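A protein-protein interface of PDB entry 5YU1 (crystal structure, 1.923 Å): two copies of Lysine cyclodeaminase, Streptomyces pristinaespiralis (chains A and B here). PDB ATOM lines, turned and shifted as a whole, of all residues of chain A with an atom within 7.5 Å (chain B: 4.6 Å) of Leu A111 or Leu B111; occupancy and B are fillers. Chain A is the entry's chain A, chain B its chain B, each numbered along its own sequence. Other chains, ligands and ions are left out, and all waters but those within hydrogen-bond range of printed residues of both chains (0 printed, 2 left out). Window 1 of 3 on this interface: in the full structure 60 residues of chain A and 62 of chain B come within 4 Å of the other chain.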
ATOM      1  N   THR A   3     -34.409 -21.932  -6.627  1.00  0.00           N
ATOM      2  CA  THR A   3     -32.995 -22.136  -6.353  1.00  0.00           C
ATOM      3  C   THR A   3     -32.145 -21.325  -7.326  1.00  0.00           C
ATOM      4  O   THR A   3     -32.386 -21.339  -8.538  1.00  0.00           O
ATOM      5  CB  THR A   3     -32.651 -23.617  -6.465  1.00  0.00           C
ATOM      6  OG1 THR A   3     -33.413 -24.342  -5.498  1.00  0.00           O
ATOM      7  CG2 THR A   3     -31.142 -23.858  -6.222  1.00  0.00           C
ATOM      8  N   TRP A   4     -31.143 -20.638  -6.791  1.00  0.00           N
ATOM      9  CA  TRP A   4     -30.192 -19.885  -7.602  1.00  0.00           C
ATOM     10  C   TRP A   4     -29.096 -20.843  -8.046  1.00  0.00           C
ATOM     11  O   TRP A   4     -28.317 -21.329  -7.222  1.00  0.00           O
ATOM     12  CB  TRP A   4     -29.633 -18.724  -6.787  1.00  0.00           C
ATOM     13  CG  TRP A   4     -28.688 -17.808  -7.508  1.00  0.00           C
ATOM     14  CD1 TRP A   4     -28.553 -17.639  -8.861  1.00  0.00           C
ATOM     15  CD2 TRP A   4     -27.758 -16.915  -6.892  1.00  0.00           C
ATOM     16  NE1 TRP A   4     -27.581 -16.683  -9.120  1.00  0.00           N
ATOM     17  CE2 TRP A   4     -27.077 -16.233  -7.927  1.00  0.00           C
ATOM     18  CE3 TRP A   4     -27.420 -16.636  -5.560  1.00  0.00           C
ATOM     19  CZ2 TRP A   4     -26.089 -15.282  -7.669  1.00  0.00           C
ATOM     20  CZ3 TRP A   4     -26.432 -15.696  -5.304  1.00  0.00           C
ATOM     21  CH2 TRP A   4     -25.780 -15.028  -6.355  1.00  0.00           C
ATOM     22  N   VAL A   5     -29.050 -21.157  -9.332  1.00  0.00           N
ATOM     23  CA  VAL A   5     -28.068 -22.096  -9.852  1.00  0.00           C
ATOM     24  C   VAL A   5     -27.001 -21.307 -10.595  1.00  0.00           C
ATOM     25  O   VAL A   5     -27.311 -20.531 -11.503  1.00  0.00           O
ATOM     26  CB  VAL A   5     -28.710 -23.153 -10.760  1.00  0.00           C
ATOM     27  CG1 VAL A   5     -27.628 -24.121 -11.291  1.00  0.00           C
ATOM     28  CG2 VAL A   5     -29.790 -23.919  -9.992  1.00  0.00           C
ATOM     29  N   LEU A   6     -25.753 -21.489 -10.193  1.00  0.00           N
ATOM     30  CA  LEU A   6     -24.599 -20.949 -10.908  1.00  0.00           C
ATOM     31  C   LEU A   6     -23.954 -22.104 -11.663  1.00  0.00           C
ATOM     32  O   LEU A   6     -23.191 -22.879 -11.084  1.00  0.00           O
ATOM     33  CB  LEU A   6     -23.604 -20.317  -9.947  1.00  0.00           C
ATOM     34  CG  LEU A   6     -23.950 -19.047  -9.178  1.00  0.00           C
ATOM     35  CD1 LEU A   6     -22.745 -18.650  -8.325  1.00  0.00           C
ATOM     36  CD2 LEU A   6     -24.308 -17.942 -10.142  1.00  0.00           C
ATOM     37  N   GLY A   7     -24.251 -22.220 -12.951  1.00  0.00           N
ATOM     38  CA  GLY A   7     -23.656 -23.263 -13.757  1.00  0.00           C
ATOM     39  C   GLY A   7     -22.194 -22.988 -14.065  1.00  0.00           C
ATOM     40  O   GLY A   7     -21.613 -21.977 -13.667  1.00  0.00           O
ATOM     41  N   VAL A  11     -19.770 -19.610 -13.293  1.00  0.00           N
ATOM     42  CA  VAL A  11     -18.512 -19.627 -12.557  1.00  0.00           C
ATOM     43  C   VAL A  11     -17.366 -19.151 -13.448  1.00  0.00           C
ATOM     44  O   VAL A  11     -16.496 -18.392 -13.007  1.00  0.00           O
ATOM     45  CB  VAL A  11     -18.245 -21.031 -11.986  1.00  0.00           C
ATOM     46  CG1 VAL A  11     -16.872 -21.092 -11.407  1.00  0.00           C
ATOM     47  CG2 VAL A  11     -19.288 -21.368 -10.902  1.00  0.00           C
ATOM     48  N   LEU A  76     -23.328 -27.445   2.043  1.00  0.00           N
ATOM     49  CA  LEU A  76     -22.936 -28.838   1.853  1.00  0.00           C
ATOM     50  C   LEU A  76     -22.124 -28.964   0.576  1.00  0.00           C
ATOM     51  O   LEU A  76     -22.626 -28.662  -0.513  1.00  0.00           O
ATOM     52  CB  LEU A  76     -24.154 -29.764   1.783  1.00  0.00           C
ATOM     53  CG  LEU A  76     -23.738 -31.241   1.759  1.00  0.00           C
ATOM     54  CD1 LEU A  76     -23.354 -31.724   3.158  1.00  0.00           C
ATOM     55  CD2 LEU A  76     -24.839 -32.112   1.178  1.00  0.00           C
ATOM     56  N   THR A  78     -20.406 -31.822  -1.800  1.00  0.00           N
ATOM     57  CA  THR A  78     -20.294 -33.227  -2.155  1.00  0.00           C
ATOM     58  C   THR A  78     -19.174 -33.316  -3.177  1.00  0.00           C
ATOM     59  O   THR A  78     -19.152 -32.532  -4.132  1.00  0.00           O
ATOM     60  CB  THR A  78     -21.610 -33.758  -2.737  1.00  0.00           C
ATOM     61  OG1 THR A  78     -22.049 -32.890  -3.790  1.00  0.00           O
ATOM     62  CG2 THR A  78     -22.707 -33.815  -1.658  1.00  0.00           C
ATOM     63  N   THR A  97     -19.725 -30.481  -6.201  1.00  0.00           N
ATOM     64  CA  THR A  97     -20.669 -29.375  -6.249  1.00  0.00           C
ATOM     65  C   THR A  97     -20.893 -28.884  -4.827  1.00  0.00           C
ATOM     66  O   THR A  97     -20.632 -29.599  -3.857  1.00  0.00           O
ATOM     67  CB  THR A  97     -21.989 -29.803  -6.905  1.00  0.00           C
ATOM     68  OG1 THR A  97     -22.302 -31.135  -6.495  1.00  0.00           O
ATOM     69  CG2 THR A  97     -21.868 -29.788  -8.443  1.00  0.00           C
ATOM     70  N   VAL A  98     -21.349 -27.639  -4.700  1.00  0.00           N
ATOM     71  CA  VAL A  98     -21.539 -26.995  -3.404  1.00  0.00           C
ATOM     72  C   VAL A  98     -22.948 -26.422  -3.369  1.00  0.00           C
ATOM     73  O   VAL A  98     -23.355 -25.706  -4.294  1.00  0.00           O
ATOM     74  CB  VAL A  98     -20.510 -25.873  -3.143  1.00  0.00           C
ATOM     75  CG1 VAL A  98     -20.444 -25.541  -1.647  1.00  0.00           C
ATOM     76  CG2 VAL A  98     -19.124 -26.265  -3.659  1.00  0.00           C
ATOM     77  N   ALA A  99     -23.678 -26.709  -2.298  1.00  0.00           N
ATOM     78  CA  ALA A  99     -25.060 -26.268  -2.160  1.00  0.00           C
ATOM     79  C   ALA A  99     -25.217 -25.442  -0.897  1.00  0.00           C
ATOM     80  O   ALA A  99     -24.500 -25.643   0.092  1.00  0.00           O
ATOM     81  CB  ALA A  99     -26.033 -27.466  -2.127  1.00  0.00           C
ATOM     82  N   ARG A 100     -26.176 -24.512  -0.934  1.00  0.00           N
ATOM     83  CA  ARG A 100     -26.512 -23.692   0.218  1.00  0.00           C
ATOM     84  C   ARG A 100     -28.001 -23.831   0.529  1.00  0.00           C
ATOM     85  O   ARG A 100     -28.844 -23.794  -0.375  1.00  0.00           O
ATOM     86  CB  ARG A 100     -26.144 -22.217  -0.014  1.00  0.00           C
ATOM     87  CG  ARG A 100     -26.374 -21.357   1.217  1.00  0.00           C
ATOM     88  CD  ARG A 100     -25.790 -19.963   1.062  1.00  0.00           C
ATOM     89  NE  ARG A 100     -24.336 -19.955   1.228  1.00  0.00           N
ATOM     90  CZ  ARG A 100     -23.619 -18.852   1.423  1.00  0.00           C
ATOM     91  NH1 ARG A 100     -24.233 -17.683   1.491  1.00  0.00           N
ATOM     92  NH2 ARG A 100     -22.295 -18.925   1.566  1.00  0.00           N
ATOM     93  N   TYR A 101     -28.308 -24.007   1.810  1.00  0.00           N
ATOM     94  CA  TYR A 101     -29.665 -24.231   2.297  1.00  0.00           C
ATOM     95  C   TYR A 101     -29.991 -23.180   3.340  1.00  0.00           C
ATOM     96  O   TYR A 101     -29.142 -22.840   4.170  1.00  0.00           O
ATOM     97  CB  TYR A 101     -29.823 -25.634   2.919  1.00  0.00           C
ATOM     98  CG  TYR A 101     -29.462 -26.737   1.975  1.00  0.00           C
ATOM     99  CD1 TYR A 101     -28.131 -27.102   1.784  1.00  0.00           C
ATOM    100  CD2 TYR A 101     -30.447 -27.412   1.252  1.00  0.00           C
ATOM    101  CE1 TYR A 101     -27.792 -28.117   0.906  1.00  0.00           C
ATOM    102  CE2 TYR A 101     -30.114 -28.430   0.371  1.00  0.00           C
ATOM    103  CZ  TYR A 101     -28.785 -28.775   0.199  1.00  0.00           C
ATOM    104  OH  TYR A 101     -28.431 -29.774  -0.684  1.00  0.00           O
ATOM    105  N   LEU A 108     -33.426 -25.239  -0.345  1.00  0.00           N
ATOM    106  CA  LEU A 108     -32.228 -25.158  -1.184  1.00  0.00           C
ATOM    107  C   LEU A 108     -32.194 -23.804  -1.892  1.00  0.00           C
ATOM    108  O   LEU A 108     -33.001 -23.547  -2.793  1.00  0.00           O
ATOM    109  CB  LEU A 108     -32.215 -26.294  -2.199  1.00  0.00           C
ATOM    110  CG  LEU A 108     -31.137 -26.198  -3.280  1.00  0.00           C
ATOM    111  CD1 LEU A 108     -29.717 -26.396  -2.687  1.00  0.00           C
ATOM    112  CD2 LEU A 108     -31.413 -27.201  -4.400  1.00  0.00           C
ATOM    113  N   THR A 109     -31.259 -22.932  -1.497  1.00  0.00           N
ATOM    114  CA  THR A 109     -31.244 -21.574  -2.037  1.00  0.00           C
ATOM    115  C   THR A 109     -30.201 -21.348  -3.126  1.00  0.00           C
ATOM    116  O   THR A 109     -30.390 -20.447  -3.954  1.00  0.00           O
ATOM    117  CB  THR A 109     -31.035 -20.545  -0.916  1.00  0.00           C
ATOM    118  OG1 THR A 109     -29.806 -20.802  -0.220  1.00  0.00           O
ATOM    119  CG2 THR A 109     -32.210 -20.587   0.087  1.00  0.00           C
ATOM    120  N   ALA A 110     -29.119 -22.134  -3.161  1.00  0.00           N
ATOM    121  CA  ALA A 110     -28.089 -21.922  -4.174  1.00  0.00           C
ATOM    122  C   ALA A 110     -27.301 -23.206  -4.396  1.00  0.00           C
ATOM    123  O   ALA A 110     -27.123 -24.008  -3.475  1.00  0.00           O
ATOM    124  CB  ALA A 110     -27.141 -20.787  -3.777  1.00  0.00           C
ATOM    125  N   LEU A 111     -26.825 -23.375  -5.628  1.00  0.00           N
ATOM    126  CA  LEU A 111     -26.104 -24.568  -6.053  1.00  0.00           C
ATOM    127  C   LEU A 111     -25.075 -24.167  -7.101  1.00  0.00           C
ATOM    128  O   LEU A 111     -25.419 -23.476  -8.061  1.00  0.00           O
ATOM    129  CB  LEU A 111     -27.073 -25.601  -6.630  1.00  0.00           C
ATOM    130  CG  LEU A 111     -26.468 -26.839  -7.276  1.00  0.00           C
ATOM    131  CD1 LEU A 111     -25.739 -27.675  -6.222  1.00  0.00           C
ATOM    132  CD2 LEU A 111     -27.564 -27.652  -7.951  1.00  0.00           C
ATOM    133  N   MET A 112     -23.824 -24.603  -6.934  1.00  0.00           N
ATOM    134  CA  MET A 112     -22.786 -24.197  -7.872  1.00  0.00           C
ATOM    135  C   MET A 112     -21.755 -25.302  -8.039  1.00  0.00           C
ATOM    136  O   MET A 112     -21.659 -26.226  -7.219  1.00  0.00           O
ATOM    137  CB  MET A 112     -22.105 -22.895  -7.419  1.00  0.00           C
ATOM    138  CG  MET A 112     -21.289 -23.031  -6.116  1.00  0.00           C
ATOM    139  SD  MET A 112     -20.364 -21.513  -5.707  1.00  0.00           S
ATOM    140  CE  MET A 112     -19.157 -21.513  -7.030  1.00  0.00           C
ATOM    141  N   ASP A 113     -20.992 -25.197  -9.132  1.00  0.00           N
ATOM    142  CA  ASP A 113     -19.824 -26.046  -9.345  1.00  0.00           C
ATOM    143  C   ASP A 113     -18.903 -26.023  -8.134  1.00  0.00           C
ATOM    144  O   ASP A 113     -18.725 -24.985  -7.493  1.00  0.00           O
ATOM    145  CB  ASP A 113     -19.026 -25.578 -10.563  1.00  0.00           C
ATOM    146  CG  ASP A 113     -17.670 -26.262 -10.664  1.00  0.00           C
ATOM    147  OD1 ASP A 113     -17.652 -27.507 -10.825  1.00  0.00           O
ATOM    148  OD2 ASP A 113     -16.628 -25.564 -10.579  1.00  0.00           O
ATOM    149  N   GLY A 114     -18.285 -27.167  -7.853  1.00  0.00           N
ATOM    150  CA  GLY A 114     -17.287 -27.241  -6.808  1.00  0.00           C
ATOM    151  C   GLY A 114     -15.891 -27.569  -7.309  1.00  0.00           C
ATOM    152  O   GLY A 114     -14.952 -27.597  -6.512  1.00  0.00           O
ATOM    153  N   MET A 312     -17.492 -20.143  -1.396  1.00  0.00           N
ATOM    154  CA  MET A 312     -18.790 -19.990  -2.048  1.00  0.00           C
ATOM    155  C   MET A 312     -19.344 -18.585  -1.827  1.00  0.00           C
ATOM    156  O   MET A 312     -19.926 -17.989  -2.743  1.00  0.00           O
ATOM    157  CB  MET A 312     -19.774 -21.050  -1.540  1.00  0.00           C
ATOM    158  CG  MET A 312     -21.215 -20.879  -2.101  1.00  0.00           C
ATOM    159  SD  MET A 312     -22.108 -22.462  -2.061  1.00  0.00           S
ATOM    160  CE  MET A 312     -23.553 -22.128  -3.084  1.00  0.00           C
ATOM    161  N   LEU A 316     -20.595 -16.023  -4.623  1.00  0.00           N
ATOM    162  CA  LEU A 316     -21.978 -15.542  -4.618  1.00  0.00           C
ATOM    163  C   LEU A 316     -22.040 -14.022  -4.586  1.00  0.00           C
ATOM    164  O   LEU A 316     -22.922 -13.422  -5.210  1.00  0.00           O
ATOM    165  CB  LEU A 316     -22.740 -16.118  -3.422  1.00  0.00           C
ATOM    166  CG  LEU A 316     -23.016 -17.628  -3.441  1.00  0.00           C
ATOM    167  CD1 LEU A 316     -23.937 -18.004  -2.295  1.00  0.00           C
ATOM    168  CD2 LEU A 316     -23.595 -18.093  -4.766  1.00  0.00           C
ATOM    169  N   ILE A 326     -28.963 -18.703 -12.976  1.00  0.00           N
ATOM    170  CA  ILE A 326     -30.363 -18.880 -13.338  1.00  0.00           C
ATOM    171  C   ILE A 326     -31.161 -19.246 -12.094  1.00  0.00           C
ATOM    172  O   ILE A 326     -30.611 -19.630 -11.057  1.00  0.00           O
ATOM    173  CB  ILE A 326     -30.562 -19.951 -14.437  1.00  0.00           C
ATOM    174  CG1 ILE A 326     -30.010 -21.306 -13.975  1.00  0.00           C
ATOM    175  CG2 ILE A 326     -29.915 -19.504 -15.757  1.00  0.00           C
ATOM    176  CD1 ILE A 326     -30.428 -22.464 -14.862  1.00  0.00           C
ATOM    177  N   VAL A 328     -34.147 -21.784 -10.815  1.00  0.00           N
ATOM    178  CA  VAL A 328     -34.845 -23.024 -11.141  1.00  0.00           C
ATOM    179  C   VAL A 328     -35.714 -23.418  -9.949  1.00  0.00           C
ATOM    180  O   VAL A 328     -35.214 -23.550  -8.826  1.00  0.00           O
ATOM    181  CB  VAL A 328     -33.874 -24.165 -11.503  1.00  0.00           C
ATOM    182  CG1 VAL A 328     -34.648 -25.378 -11.995  1.00  0.00           C
ATOM    183  CG2 VAL A 328     -32.870 -23.730 -12.563  1.00  0.00           C
ATOM    184  N   ILE A 330     -36.829 -26.107  -8.158  1.00  0.00           N
ATOM    185  CA  ILE A 330     -36.507 -27.525  -8.039  1.00  0.00           C
ATOM    186  C   ILE A 330     -37.426 -28.144  -6.995  1.00  0.00           C
ATOM    187  O   ILE A 330     -38.145 -29.109  -7.275  1.00  0.00           O
ATOM    188  CB  ILE A 330     -35.028 -27.750  -7.666  1.00  0.00           C
ATOM    189  CG1 ILE A 330     -34.101 -27.001  -8.636  1.00  0.00           C
ATOM    190  CG2 ILE A 330     -34.717 -29.261  -7.639  1.00  0.00           C
ATOM    191  CD1 ILE A 330     -32.602 -27.133  -8.306  1.00  0.00           C
ATOM    192  N   THR B   3     -26.127 -32.051 -16.163  1.00  0.00           N
ATOM    193  CA  THR B   3     -27.006 -32.582 -15.129  1.00  0.00           C
ATOM    194  C   THR B   3     -28.465 -32.520 -15.571  1.00  0.00           C
ATOM    195  O   THR B   3     -28.942 -31.478 -16.032  1.00  0.00           O
ATOM    196  CB  THR B   3     -26.836 -31.792 -13.833  1.00  0.00           C
ATOM    197  OG1 THR B   3     -25.477 -31.901 -13.391  1.00  0.00           O
ATOM    198  CG2 THR B   3     -27.785 -32.333 -12.745  1.00  0.00           C
ATOM    199  N   TRP B   4     -29.170 -33.635 -15.408  1.00  0.00           N
ATOM    200  CA  TRP B   4     -30.600 -33.700 -15.682  1.00  0.00           C
ATOM    201  C   TRP B   4     -31.354 -33.189 -14.458  1.00  0.00           C
ATOM    202  O   TRP B   4     -31.233 -33.752 -13.365  1.00  0.00           O
ATOM    203  CB  TRP B   4     -30.977 -35.142 -16.031  1.00  0.00           C
ATOM    204  CG  TRP B   4     -32.401 -35.381 -16.464  1.00  0.00           C
ATOM    205  CD1 TRP B   4     -33.304 -34.461 -16.926  1.00  0.00           C
ATOM    206  CD2 TRP B   4     -33.068 -36.646 -16.481  1.00  0.00           C
ATOM    207  NE1 TRP B   4     -34.495 -35.084 -17.228  1.00  0.00           N
ATOM    208  CE2 TRP B   4     -34.376 -36.424 -16.962  1.00  0.00           C
ATOM    209  CE3 TRP B   4     -32.682 -37.948 -16.144  1.00  0.00           C
ATOM    210  CZ2 TRP B   4     -35.306 -37.460 -17.103  1.00  0.00           C
ATOM    211  CZ3 TRP B   4     -33.605 -38.975 -16.282  1.00  0.00           C
ATOM    212  CH2 TRP B   4     -34.901 -38.723 -16.755  1.00  0.00           C
ATOM    213  N   VAL B   5     -32.089 -32.096 -14.608  1.00  0.00           N
ATOM    214  CA  VAL B   5     -32.797 -31.487 -13.486  1.00  0.00           C
ATOM    215  C   VAL B   5     -34.291 -31.654 -13.707  1.00  0.00           C
ATOM    216  O   VAL B   5     -34.833 -31.196 -14.723  1.00  0.00           O
ATOM    217  CB  VAL B   5     -32.420 -30.010 -13.301  1.00  0.00           C
ATOM    218  CG1 VAL B   5     -33.183 -29.416 -12.111  1.00  0.00           C
ATOM    219  CG2 VAL B   5     -30.907 -29.885 -13.083  1.00  0.00           C
ATOM    220  N   LEU B   6     -34.944 -32.329 -12.763  1.00  0.00           N
ATOM    221  CA  LEU B   6     -36.401 -32.439 -12.719  1.00  0.00           C
ATOM    222  C   LEU B   6     -36.899 -31.436 -11.690  1.00  0.00           C
ATOM    223  O   LEU B   6     -36.807 -31.676 -10.484  1.00  0.00           O
ATOM    224  CB  LEU B   6     -36.840 -33.849 -12.352  1.00  0.00           C
ATOM    225  CG  LEU B   6     -36.448 -35.003 -13.261  1.00  0.00           C
ATOM    226  CD1 LEU B   6     -37.084 -36.290 -12.737  1.00  0.00           C
ATOM    227  CD2 LEU B   6     -36.900 -34.719 -14.685  1.00  0.00           C
ATOM    228  N   THR B  97     -34.375 -32.263  -1.388  1.00  0.00           N
ATOM    229  CA  THR B  97     -33.997 -32.501  -2.771  1.00  0.00           C
ATOM    230  C   THR B  97     -33.142 -33.762  -2.806  1.00  0.00           C
ATOM    231  O   THR B  97     -32.548 -34.166  -1.800  1.00  0.00           O
ATOM    232  CB  THR B  97     -33.217 -31.308  -3.381  1.00  0.00           C
ATOM    233  OG1 THR B  97     -32.230 -30.857  -2.449  1.00  0.00           O
ATOM    234  CG2 THR B  97     -34.134 -30.137  -3.694  1.00  0.00           C
ATOM    235  N   VAL B  98     -33.091 -34.395  -3.969  1.00  0.00           N
ATOM    236  CA  VAL B  98     -32.394 -35.666  -4.123  1.00  0.00           C
ATOM    237  C   VAL B  98     -31.468 -35.571  -5.327  1.00  0.00           C
ATOM    238  O   VAL B  98     -31.897 -35.184  -6.420  1.00  0.00           O
ATOM    239  CB  VAL B  98     -33.378 -36.840  -4.285  1.00  0.00           C
ATOM    240  CG1 VAL B  98     -32.638 -38.152  -4.103  1.00  0.00           C
ATOM    241  CG2 VAL B  98     -34.542 -36.719  -3.288  1.00  0.00           C
ATOM    242  N   ALA B  99     -30.203 -35.933  -5.132  1.00  0.00           N
ATOM    243  CA  ALA B  99     -29.195 -35.854  -6.178  1.00  0.00           C
ATOM    244  C   ALA B  99     -28.654 -37.244  -6.476  1.00  0.00           C
ATOM    245  O   ALA B  99     -28.552 -38.091  -5.583  1.00  0.00           O
ATOM    246  CB  ALA B  99     -28.043 -34.916  -5.764  1.00  0.00           C
ATOM    247  N   ALA B 110     -28.029 -36.216 -11.965  1.00  0.00           N
ATOM    248  CA  ALA B 110     -29.453 -35.903 -11.884  1.00  0.00           C
ATOM    249  C   ALA B 110     -29.761 -35.209 -10.563  1.00  0.00           C
ATOM    250  O   ALA B 110     -29.096 -35.450  -9.556  1.00  0.00           O
ATOM    251  CB  ALA B 110     -30.301 -37.178 -12.032  1.00  0.00           C
ATOM    252  N   LEU B 111     -30.781 -34.348 -10.582  1.00  0.00           N
ATOM    253  CA  LEU B 111     -31.216 -33.614  -9.398  1.00  0.00           C
ATOM    254  C   LEU B 111     -32.718 -33.378  -9.476  1.00  0.00           C
ATOM    255  O   LEU B 111     -33.208 -32.908 -10.509  1.00  0.00           O
ATOM    256  CB  LEU B 111     -30.494 -32.271  -9.293  1.00  0.00           C
ATOM    257  CG  LEU B 111     -30.899 -31.395  -8.115  1.00  0.00           C
ATOM    258  CD1 LEU B 111     -30.442 -32.013  -6.783  1.00  0.00           C
ATOM    259  CD2 LEU B 111     -30.306 -30.001  -8.314  1.00  0.00           C
ATOM    260  N   MET B 112     -33.445 -33.667  -8.396  1.00  0.00           N
ATOM    261  CA  MET B 112     -34.898 -33.480  -8.426  1.00  0.00           C
ATOM    262  C   MET B 112     -35.435 -33.064  -7.064  1.00  0.00           C
ATOM    263  O   MET B 112     -34.759 -33.168  -6.034  1.00  0.00           O
ATOM    264  CB  MET B 112     -35.621 -34.755  -8.891  1.00  0.00           C
ATOM    265  CG  MET B 112     -35.435 -35.957  -7.968  1.00  0.00           C
ATOM    266  SD  MET B 112     -36.444 -37.389  -8.449  1.00  0.00           S
ATOM    267  CE  MET B 112     -38.075 -36.662  -8.397  1.00  0.00           C
ATOM    268  N   MET B 312     -36.573 -42.322  -6.510  1.00  0.00           N
ATOM    269  CA  MET B 312     -36.017 -41.499  -7.579  1.00  0.00           C
ATOM    270  C   MET B 312     -35.963 -42.268  -8.899  1.00  0.00           C
ATOM    271  O   MET B 312     -36.242 -41.706  -9.963  1.00  0.00           O
ATOM    272  CB  MET B 312     -34.624 -41.004  -7.184  1.00  0.00           C
ATOM    273  CG  MET B 312     -33.956 -40.159  -8.255  1.00  0.00           C
ATOM    274  SD  MET B 312     -32.739 -39.055  -7.523  1.00  0.00           S
ATOM    275  CE  MET B 312     -32.307 -37.982  -8.908  1.00  0.00           C
ATOM    276  N   ILE B 330     -23.701 -27.867 -14.638  1.00  0.00           N
ATOM    277  CA  ILE B 330     -23.417 -27.347 -13.304  1.00  0.00           C
ATOM    278  C   ILE B 330     -21.943 -27.541 -12.977  1.00  0.00           C
ATOM    279  O   ILE B 330     -21.243 -26.584 -12.614  1.00  0.00           O
ATOM    280  CB  ILE B 330     -24.306 -28.026 -12.248  1.00  0.00           C
ATOM    281  CG1 ILE B 330     -25.788 -27.815 -12.597  1.00  0.00           C
ATOM    282  CG2 ILE B 330     -23.971 -27.505 -10.840  1.00  0.00           C
ATOM    283  CD1 ILE B 330     -26.736 -28.532 -11.655  1.00  0.00           C
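Thr A97 touches Ile B330, but with the chains exchanged Ile A330 does not touch Thr B97 (4.1 Å).
Leu A111 touches its own counterpart, Leu B111.
Leu A111 touches Ile B330, and with the chains exchanged Ile A330 touches Leu B111.
Ile A330 touches Met B112, but with the chains exchanged Met A112 does not touch Ile B330 (4.2 Å).
Positions printed for both chains: 3, 4, 5, 6, 97, 98, 99, 110, 111, 112, 312 and 330.
Among the printed residues, pairs that only touch across the chains: Gly A7 with Ile B330 (3.99 Å), Thr A97 with Ile B330 (3.9 Å), Leu A111 with Leu B111 (3.6 Å), Leu A111 with Ile B330 (3.9 Å), Asp A113 with Ile B330 (3.2 Å), Ile A330 with Leu B111 (3.7 Å) and Ile A330 with Met B112 (3.9 Å).
Of the 12 printed residues of chain B, 3 touch a printed residue of chain A.
Along chain B the printed residues that touch a printed residue of chain A span positions 111 to 330.
Along chain A the printed residues that touch a printed residue of chain B span positions 7 to 330.
Among the printed residues, no Asp or Glu carboxylate lies within 4 Å of a Lys or Arg side-chain nitrogen of the other chain.
Printed residues of chain B within 4 Å of Gly A7: Ile B330 (3.99 Å).
Thr A78 touches none of the printed residues of chain B.
Printed residues of chain B within 4 Å of Thr A97: Ile B330 (3.9 Å).
Leu A111 touches just these residues of chain B: Leu B111 and Ile B330.
Of the printed residues of chain B, Asp A113 touches Ile B330 (3.2 Å).
Printed residues of chain B within 4 Å of Ile A330: Leu B111 (3.7 Å) and Met B112 (3.9 Å).
Val B5 touches none of the printed residues of chain A.
Printed residues of chain A within 4 Å of Met B112: Ile A330.
The nearest residue of chain A that does not touch Leu B111 is Leu A108 (4.9 Å).
The backbone NH of Leu B6 sits at hydrogen-bond distance from the backbone carbonyl oxygen of Leu B111 (2.9 Å).
O of Trp A4 is in hydrogen-bond range of N of Leu A111, at 3.0 Å.
N of Leu A6 sits at hydrogen-bond distance from O of Leu A111 (2.9 Å).
N of Val B98 is in hydrogen-bond range of O of Met B112.
O of Thr A78 sits at hydrogen-bond distance from N of Thr A97 (3.0 Å).
The backbone carbonyl oxygen (O) of Trp B4 lies within hydrogen-bond range of the backbone NH (N) of Leu B111.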
